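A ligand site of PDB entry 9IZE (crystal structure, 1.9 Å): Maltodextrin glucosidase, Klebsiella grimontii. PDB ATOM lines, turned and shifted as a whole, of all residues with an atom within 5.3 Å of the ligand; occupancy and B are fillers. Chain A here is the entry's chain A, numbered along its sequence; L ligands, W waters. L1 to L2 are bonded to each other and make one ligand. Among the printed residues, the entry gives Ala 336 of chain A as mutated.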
ATOM      1  N   PHE A 129      -2.621  -5.469   2.960  1.00  0.00           N
ATOM      2  CA  PHE A 129      -3.882  -5.689   2.255  1.00  0.00           C
ATOM      3  C   PHE A 129      -4.744  -6.530   3.198  1.00  0.00           C
ATOM      4  O   PHE A 129      -4.526  -7.742   3.307  1.00  0.00           O
ATOM      5  CB  PHE A 129      -3.611  -6.392   0.915  1.00  0.00           C
ATOM      6  CG  PHE A 129      -4.797  -6.461  -0.012  1.00  0.00           C
ATOM      7  CD1 PHE A 129      -5.039  -5.451  -0.939  1.00  0.00           C
ATOM      8  CD2 PHE A 129      -5.633  -7.563   0.003  1.00  0.00           C
ATOM      9  CE1 PHE A 129      -6.116  -5.529  -1.809  1.00  0.00           C
ATOM     10  CE2 PHE A 129      -6.710  -7.657  -0.863  1.00  0.00           C
ATOM     11  CZ  PHE A 129      -6.951  -6.632  -1.771  1.00  0.00           C
ATOM     12  N   GLY A 170     -11.511 -12.084  -9.012  1.00  0.00           N
ATOM     13  CA  GLY A 170     -10.365 -11.524  -8.320  1.00  0.00           C
ATOM     14  C   GLY A 170     -10.736 -10.460  -7.306  1.00  0.00           C
ATOM     15  O   GLY A 170     -10.091 -10.336  -6.262  1.00  0.00           O
ATOM     16  N   GLY A 171     -11.764  -9.663  -7.606  1.00  0.00           N
ATOM     17  CA  GLY A 171     -12.257  -8.626  -6.731  1.00  0.00           C
ATOM     18  C   GLY A 171     -13.338  -9.056  -5.762  1.00  0.00           C
ATOM     19  O   GLY A 171     -13.847  -8.218  -5.011  1.00  0.00           O
ATOM     20  N   HIS A 209     -10.867  -5.647  -2.241  1.00  0.00           N
ATOM     21  CA  HIS A 209      -9.852  -4.591  -2.134  1.00  0.00           C
ATOM     22  C   HIS A 209     -10.436  -3.303  -1.571  1.00  0.00           C
ATOM     23  O   HIS A 209      -9.692  -2.509  -0.967  1.00  0.00           O
ATOM     24  CB  HIS A 209      -9.233  -4.314  -3.505  1.00  0.00           C
ATOM     25  CG  HIS A 209     -10.239  -4.082  -4.579  1.00  0.00           C
ATOM     26  ND1 HIS A 209     -10.960  -2.912  -4.696  1.00  0.00           N
ATOM     27  CD2 HIS A 209     -10.682  -4.894  -5.570  1.00  0.00           C
ATOM     28  CE1 HIS A 209     -11.781  -2.999  -5.720  1.00  0.00           C
ATOM     29  NE2 HIS A 209     -11.640  -4.199  -6.268  1.00  0.00           N
ATOM     30  N   TYR A 211     -11.533  -0.480  -2.889  1.00  0.00           N
ATOM     31  CA  TYR A 211     -11.388   0.827  -3.542  1.00  0.00           C
ATOM     32  C   TYR A 211     -12.712   1.311  -4.125  1.00  0.00           C
ATOM     33  O   TYR A 211     -12.781   2.446  -4.618  1.00  0.00           O
ATOM     34  CB  TYR A 211     -10.312   0.753  -4.611  1.00  0.00           C
ATOM     35  CG  TYR A 211      -8.927   0.702  -4.034  1.00  0.00           C
ATOM     36  CD1 TYR A 211      -8.302   1.865  -3.576  1.00  0.00           C
ATOM     37  CD2 TYR A 211      -8.247  -0.497  -3.909  1.00  0.00           C
ATOM     38  CE1 TYR A 211      -7.021   1.830  -3.020  1.00  0.00           C
ATOM     39  CE2 TYR A 211      -6.967  -0.549  -3.349  1.00  0.00           C
ATOM     40  CZ  TYR A 211      -6.364   0.611  -2.909  1.00  0.00           C
ATOM     41  OH  TYR A 211      -5.099   0.566  -2.376  1.00  0.00           O
ATOM     42  N   VAL A 248      -9.338   7.242  -0.857  1.00  0.00           N
ATOM     43  CA  VAL A 248      -9.744   7.027  -2.237  1.00  0.00           C
ATOM     44  C   VAL A 248     -10.749   8.094  -2.621  1.00  0.00           C
ATOM     45  O   VAL A 248     -11.968   7.912  -2.465  1.00  0.00           O
ATOM     46  CB  VAL A 248     -10.295   5.604  -2.428  1.00  0.00           C
ATOM     47  CG1 VAL A 248     -10.415   5.255  -3.904  1.00  0.00           C
ATOM     48  CG2 VAL A 248      -9.394   4.601  -1.724  1.00  0.00           C
ATOM     49  N   HIS A 251     -12.480   8.915  -6.966  1.00  0.00           N
ATOM     50  CA  HIS A 251     -13.725   8.259  -7.334  1.00  0.00           C
ATOM     51  C   HIS A 251     -14.304   7.617  -6.089  1.00  0.00           C
ATOM     52  O   HIS A 251     -13.593   7.369  -5.114  1.00  0.00           O
ATOM     53  CB  HIS A 251     -13.479   7.209  -8.410  1.00  0.00           C
ATOM     54  CG  HIS A 251     -12.435   6.193  -8.047  1.00  0.00           C
ATOM     55  ND1 HIS A 251     -11.126   6.294  -8.448  1.00  0.00           N
ATOM     56  CD2 HIS A 251     -12.519   5.052  -7.321  1.00  0.00           C
ATOM     57  CE1 HIS A 251     -10.442   5.251  -7.999  1.00  0.00           C
ATOM     58  NE2 HIS A 251     -11.264   4.487  -7.304  1.00  0.00           N
ATOM     59  N   TRP A 292     -13.115   5.515 -13.364  1.00  0.00           N
ATOM     60  CA  TRP A 292     -11.673   5.274 -13.314  1.00  0.00           C
ATOM     61  C   TRP A 292     -11.317   4.293 -14.410  1.00  0.00           C
ATOM     62  O   TRP A 292     -11.578   3.095 -14.311  1.00  0.00           O
ATOM     63  CB  TRP A 292     -11.231   4.764 -11.944  1.00  0.00           C
ATOM     64  CG  TRP A 292      -9.743   4.561 -11.865  1.00  0.00           C
ATOM     65  CD1 TRP A 292      -8.801   5.543 -11.716  1.00  0.00           C
ATOM     66  CD2 TRP A 292      -9.024   3.325 -11.939  1.00  0.00           C
ATOM     67  NE1 TRP A 292      -7.540   4.986 -11.685  1.00  0.00           N
ATOM     68  CE2 TRP A 292      -7.650   3.628 -11.818  1.00  0.00           C
ATOM     69  CE3 TRP A 292      -9.404   1.985 -12.092  1.00  0.00           C
ATOM     70  CZ2 TRP A 292      -6.654   2.646 -11.847  1.00  0.00           C
ATOM     71  CZ3 TRP A 292      -8.422   1.005 -12.116  1.00  0.00           C
ATOM     72  CH2 TRP A 292      -7.058   1.344 -11.998  1.00  0.00           C
ATOM     73  N   TYR A 295     -13.837   1.499 -15.507  1.00  0.00           N
ATOM     74  CA  TYR A 295     -14.452   0.564 -14.573  1.00  0.00           C
ATOM     75  C   TYR A 295     -15.713   1.218 -14.023  1.00  0.00           C
ATOM     76  O   TYR A 295     -15.631   2.184 -13.247  1.00  0.00           O
ATOM     77  CB  TYR A 295     -13.466   0.171 -13.479  1.00  0.00           C
ATOM     78  CG  TYR A 295     -12.317  -0.702 -13.989  1.00  0.00           C
ATOM     79  CD1 TYR A 295     -12.437  -2.084 -14.050  1.00  0.00           C
ATOM     80  CD2 TYR A 295     -11.118  -0.136 -14.425  1.00  0.00           C
ATOM     81  CE1 TYR A 295     -11.400  -2.891 -14.521  1.00  0.00           C
ATOM     82  CE2 TYR A 295     -10.075  -0.934 -14.904  1.00  0.00           C
ATOM     83  CZ  TYR A 295     -10.226  -2.304 -14.952  1.00  0.00           C
ATOM     84  OH  TYR A 295      -9.184  -3.082 -15.421  1.00  0.00           O
ATOM     85  N   LEU A 298     -16.401   2.353 -10.417  1.00  0.00           N
ATOM     86  CA  LEU A 298     -15.587   3.416  -9.830  1.00  0.00           C
ATOM     87  C   LEU A 298     -15.920   4.753 -10.475  1.00  0.00           C
ATOM     88  O   LEU A 298     -15.113   5.315 -11.227  1.00  0.00           O
ATOM     89  CB  LEU A 298     -14.105   3.076  -9.962  1.00  0.00           C
ATOM     90  CG  LEU A 298     -13.708   1.713  -9.381  1.00  0.00           C
ATOM     91  CD1 LEU A 298     -12.273   1.342  -9.721  1.00  0.00           C
ATOM     92  CD2 LEU A 298     -13.918   1.683  -7.869  1.00  0.00           C
ATOM     93  N   ARG A 334      -2.673   7.829   2.475  1.00  0.00           N
ATOM     94  CA  ARG A 334      -2.135   7.474   1.170  1.00  0.00           C
ATOM     95  C   ARG A 334      -3.220   7.814   0.146  1.00  0.00           C
ATOM     96  O   ARG A 334      -4.344   7.309   0.248  1.00  0.00           O
ATOM     97  CB  ARG A 334      -1.738   5.995   1.138  1.00  0.00           C
ATOM     98  CG  ARG A 334      -1.221   5.429  -0.194  1.00  0.00           C
ATOM     99  CD  ARG A 334      -2.355   5.008  -1.131  1.00  0.00           C
ATOM    100  NE  ARG A 334      -1.877   4.213  -2.251  1.00  0.00           N
ATOM    101  CZ  ARG A 334      -2.674   3.647  -3.155  1.00  0.00           C
ATOM    102  NH1 ARG A 334      -3.993   3.781  -3.085  1.00  0.00           N
ATOM    103  NH2 ARG A 334      -2.135   2.938  -4.139  1.00  0.00           N
ATOM    104  N   ALA A 336      -5.017   7.511  -3.106  1.00  0.00           N
ATOM    105  CA  ALA A 336      -5.211   6.682  -4.287  1.00  0.00           C
ATOM    106  C   ALA A 336      -5.473   7.560  -5.510  1.00  0.00           C
ATOM    107  O   ALA A 336      -6.268   8.502  -5.452  1.00  0.00           O
ATOM    108  CB  ALA A 336      -6.383   5.737  -4.072  1.00  0.00           C
ATOM    109  N   VAL A 337      -4.811   7.227  -6.623  1.00  0.00           N
ATOM    110  CA  VAL A 337      -5.037   7.898  -7.907  1.00  0.00           C
ATOM    111  C   VAL A 337      -4.940   9.409  -7.733  1.00  0.00           C
ATOM    112  O   VAL A 337      -5.764  10.168  -8.254  1.00  0.00           O
ATOM    113  CB  VAL A 337      -6.393   7.484  -8.507  1.00  0.00           C
ATOM    114  CG1 VAL A 337      -6.448   7.829 -10.015  1.00  0.00           C
ATOM    115  CG2 VAL A 337      -6.623   6.006  -8.298  1.00  0.00           C
ATOM    116  N   GLU A 373      -0.255   8.143  -4.507  1.00  0.00           N
ATOM    117  CA  GLU A 373       0.051   7.028  -5.402  1.00  0.00           C
ATOM    118  C   GLU A 373       0.511   7.580  -6.748  1.00  0.00           C
ATOM    119  O   GLU A 373      -0.294   8.144  -7.492  1.00  0.00           O
ATOM    120  CB  GLU A 373      -1.180   6.154  -5.604  1.00  0.00           C
ATOM    121  CG  GLU A 373      -0.890   4.971  -6.515  1.00  0.00           C
ATOM    122  CD  GLU A 373      -2.123   4.301  -7.098  1.00  0.00           C
ATOM    123  OE1 GLU A 373      -3.212   4.922  -7.122  1.00  0.00           O
ATOM    124  OE2 GLU A 373      -1.985   3.141  -7.546  1.00  0.00           O
ATOM    125  N   HIS A 447       0.508  -4.140  -3.919  1.00  0.00           N
ATOM    126  CA  HIS A 447      -0.701  -4.874  -4.277  1.00  0.00           C
ATOM    127  C   HIS A 447      -1.116  -4.633  -5.725  1.00  0.00           C
ATOM    128  O   HIS A 447      -2.087  -5.236  -6.200  1.00  0.00           O
ATOM    129  CB  HIS A 447      -1.834  -4.477  -3.348  1.00  0.00           C
ATOM    130  CG  HIS A 447      -2.260  -3.061  -3.497  1.00  0.00           C
ATOM    131  ND1 HIS A 447      -1.387  -2.006  -3.340  1.00  0.00           N
ATOM    132  CD2 HIS A 447      -3.454  -2.507  -3.832  1.00  0.00           C
ATOM    133  CE1 HIS A 447      -2.030  -0.864  -3.547  1.00  0.00           C
ATOM    134  NE2 HIS A 447      -3.296  -1.146  -3.847  1.00  0.00           N
ATOM    135  N   ASP A 448      -0.404  -3.748  -6.424  1.00  0.00           N
ATOM    136  CA  ASP A 448      -0.696  -3.423  -7.820  1.00  0.00           C
ATOM    137  C   ASP A 448       0.420  -3.850  -8.759  1.00  0.00           C
ATOM    138  O   ASP A 448       0.428  -3.428  -9.929  1.00  0.00           O
ATOM    139  CB  ASP A 448      -0.956  -1.914  -7.970  1.00  0.00           C
ATOM    140  CG  ASP A 448      -2.263  -1.456  -7.328  1.00  0.00           C
ATOM    141  OD1 ASP A 448      -3.246  -2.245  -7.273  1.00  0.00           O
ATOM    142  OD2 ASP A 448      -2.316  -0.281  -6.885  1.00  0.00           O
ATOM    143  N   ASN A 491       1.208 -10.362 -11.046  1.00  0.00           N
ATOM    144  CA  ASN A 491       0.436  -9.180 -10.710  1.00  0.00           C
ATOM    145  C   ASN A 491      -0.988  -9.552 -10.315  1.00  0.00           C
ATOM    146  O   ASN A 491      -1.479 -10.649 -10.618  1.00  0.00           O
ATOM    147  CB  ASN A 491       0.415  -8.197 -11.881  1.00  0.00           C
ATOM    148  CG  ASN A 491      -0.144  -6.849 -11.490  1.00  0.00           C
ATOM    149  OD1 ASN A 491      -0.048  -6.449 -10.325  1.00  0.00           O
ATOM    150  ND2 ASN A 491      -0.740  -6.141 -12.440  1.00  0.00           N
ATOM    151  N   ASP A 492      -1.624  -8.640  -9.574  1.00  0.00           N
ATOM    152  CA  ASP A 492      -3.043  -8.579  -9.260  1.00  0.00           C
ATOM    153  C   ASP A 492      -3.853  -9.407 -10.250  1.00  0.00           C
ATOM    154  O   ASP A 492      -3.894  -9.077 -11.450  1.00  0.00           O
ATOM    155  CB  ASP A 492      -3.493  -7.109  -9.286  1.00  0.00           C
ATOM    156  CG  ASP A 492      -4.931  -6.927  -8.864  1.00  0.00           C
ATOM    157  OD1 ASP A 492      -5.544  -7.871  -8.334  1.00  0.00           O
ATOM    158  OD2 ASP A 492      -5.453  -5.810  -9.060  1.00  0.00           O
ATOM    159  N   PRO A 493      -4.545 -10.470  -9.799  1.00  0.00           N
ATOM    160  CA  PRO A 493      -4.829 -10.852  -8.398  1.00  0.00           C
ATOM    161  C   PRO A 493      -3.749 -11.650  -7.692  1.00  0.00           C
ATOM    162  O   PRO A 493      -3.848 -11.851  -6.473  1.00  0.00           O
ATOM    163  CB  PRO A 493      -6.100 -11.701  -8.555  1.00  0.00           C
ATOM    164  CG  PRO A 493      -5.871 -12.430  -9.873  1.00  0.00           C
ATOM    165  CD  PRO A 493      -5.150 -11.421 -10.755  1.00  0.00           C
ATOM    166  N   ARG A 496      -1.511 -10.927  -4.157  1.00  0.00           N
ATOM    167  CA  ARG A 496      -2.233 -10.711  -2.901  1.00  0.00           C
ATOM    168  C   ARG A 496      -2.515 -12.026  -2.181  1.00  0.00           C
ATOM    169  O   ARG A 496      -3.604 -12.258  -1.674  1.00  0.00           O
ATOM    170  CB  ARG A 496      -3.517  -9.937  -3.165  1.00  0.00           C
ATOM    171  CG  ARG A 496      -3.279  -8.626  -3.921  1.00  0.00           C
ATOM    172  CD  ARG A 496      -4.548  -8.020  -4.495  1.00  0.00           C
ATOM    173  NE  ARG A 496      -4.263  -6.767  -5.200  1.00  0.00           N
ATOM    174  CZ  ARG A 496      -5.192  -5.918  -5.628  1.00  0.00           C
ATOM    175  NH1 ARG A 496      -6.489  -6.165  -5.470  1.00  0.00           N
ATOM    176  NH2 ARG A 496      -4.811  -4.785  -6.200  1.00  0.00           N
HETATM  177  C1  LIG L   1      -5.887   2.508  -6.222  1.00  0.00           C
HETATM  178  C2  LIG L   1      -5.276   1.130  -5.911  1.00  0.00           C
HETATM  179  C3  LIG L   1      -5.610   0.103  -6.920  1.00  0.00           C
HETATM  180  C4  LIG L   1      -7.039   0.242  -7.364  1.00  0.00           C
HETATM  181  C5  LIG L   1      -7.167   1.519  -8.196  1.00  0.00           C
HETATM  182  C6  LIG L   1      -8.593   1.897  -8.528  1.00  0.00           C
HETATM  183  O1  LIG L   1      -4.989   3.545  -6.159  1.00  0.00           O
HETATM  184  O2  LIG L   1      -3.855   1.163  -5.657  1.00  0.00           O
HETATM  185  O3  LIG L   1      -5.347  -1.179  -6.241  1.00  0.00           O
HETATM  186  O4  LIG L   1      -7.410  -0.924  -8.132  1.00  0.00           O
HETATM  187  O5  LIG L   1      -6.626   2.677  -7.500  1.00  0.00           O
HETATM  188  O6  LIG L   1      -9.240   2.240  -7.312  1.00  0.00           O
HETATM  189  O1  LG2 L   2      -9.659  -1.459  -8.499  1.00  0.00           O
HETATM  190  C1  LG2 L   2      -8.319  -2.958  -7.306  1.00  0.00           C
HETATM  191  C2  LG2 L   2      -7.722  -3.565  -8.497  1.00  0.00           C
HETATM  192  C3  LG2 L   2     -10.363  -5.912 -11.617  1.00  0.00           C
HETATM  193  C4  LG2 L   2      -6.282  -6.162 -13.442  1.00  0.00           C
HETATM  194  C5  LG2 L   2      -7.643  -5.667 -12.973  1.00  0.00           C
HETATM  195  C6  LG2 L   2      -7.848  -5.459 -11.406  1.00  0.00           C
HETATM  196  C7  LG2 L   2      -9.112  -4.826 -11.264  1.00  0.00           C
HETATM  197  C8  LG2 L   2      -8.454  -3.292  -9.762  1.00  0.00           C
HETATM  198  C9  LG2 L   2      -9.250  -1.966  -9.841  1.00  0.00           C
HETATM  199  C10 LG2 L   2     -10.493  -1.964 -10.663  1.00  0.00           C
HETATM  200  C11 LG2 L   2      -8.556  -1.484  -7.548  1.00  0.00           C
HETATM  201  C12 LG2 L   2     -10.088  -6.629 -12.680  1.00  0.00           C
HETATM  202  C13 LG2 L   2      -8.870  -5.886 -13.687  1.00  0.00           C
HETATM  203  N1  LG2 L   2      -9.275  -4.510  -9.908  1.00  0.00           N
HETATM  204  O2  LG2 L   2      -5.571  -6.189 -12.225  1.00  0.00           O
HETATM  205  O3  LG2 L   2      -7.334  -3.117  -6.306  1.00  0.00           O
HETATM  206  O4  LG2 L   2      -7.698  -4.999  -8.212  1.00  0.00           O
HETATM  207  O5  LG2 L   2     -10.472  -6.611 -10.346  1.00  0.00           O
HETATM  208  O6  LG2 L   2     -11.340  -6.710 -13.424  1.00  0.00           O
HETATM  209  O7  LG2 L   2      -8.551  -6.480 -14.897  1.00  0.00           O
HETATM  210  O   HOH W   1      -5.491  -1.575 -10.593  1.00  0.00           O
HETATM  211  O   HOH W   2     -13.476  -6.633 -15.550  1.00  0.00           O
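NH2 of Arg 334 lies within hydrogen-bond range of O2 of LIG L1.
An oxygen (O1) of LIG L1 is in hydrogen-bond range of the side-chain carboxylate of Glu 373, 2.4 Å away.
OH of Tyr 295 lies close to O7 of LG2 L2 (3.5 Å).
An oxygen (O2) of LIG L1 lies within hydrogen-bond range of the side-chain carboxylate (OD2) of Asp 448.
NE2 of His 447 sits at hydrogen-bond distance from O2 of LIG L1 (3.0 Å).
O3 of LG2 L2 is in hydrogen-bond range of NH2 of Arg 496 (3.0 Å).
OD2 of Asp 492 lies within hydrogen-bond range of O4 of LG2 L2, 2.5 Å away.
A ring nitrogen (NE2) of His 251 lies within hydrogen-bond range of an oxygen (O6) of LIG L1, at 3.0 Å.
An oxygen (O2) of LG2 L2 lies within hydrogen-bond range of the backbone carbonyl oxygen of Asp 492 (3.4 Å).
The backbone carbonyl oxygen of His 447 is in hydrogen-bond range of the guanidinium group of Arg 496.
The side-chain carboxylate of Asp 448 sits at hydrogen-bond distance from a ring nitrogen (NE2) of His 447, 3.3 Å away.
NH1 of Arg 334 is in hydrogen-bond range of OH of Tyr 211.
OH of Tyr 211 is in hydrogen-bond range of NE2 of His 447, 2.9 Å away.
The backbone carbonyl oxygen (O) of Leu 298 sits at hydrogen-bond distance from the backbone NH (N) of Trp 292.
The side-chain carboxylate (OE2) of Glu 373 is in salt-bridge range of the guanidinium group (NH2) of Arg 334, at 3.4 Å.
The guanidinium group of Arg 496 is in salt-bridge range of the side-chain carboxylate of Asp 492 (3.1 Å).
ND1 of His 209 is in hydrogen-bond range of N of Tyr 211.
CD2 of His 209 touches C1 of LG2 L2 (3.5 Å).
Tyr 211 touches the ligand.
Trp 292 touches the ligand.
CD1 of Leu 298 touches C10 of LG2 L2 (3.9 Å).
Ala 336 touches the ligand.
CG2 of Val 337 touches O5 of LIG L1, at 3.4 Å.
14 residues have an atom within 4 Å of the ligand: His 209, Tyr 211, His 251, Trp 292, Tyr 295, Leu 298, Arg 334, Ala 336, Val 337, Glu 373, His 447, Asp 448, Asp 492 and Arg 496.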
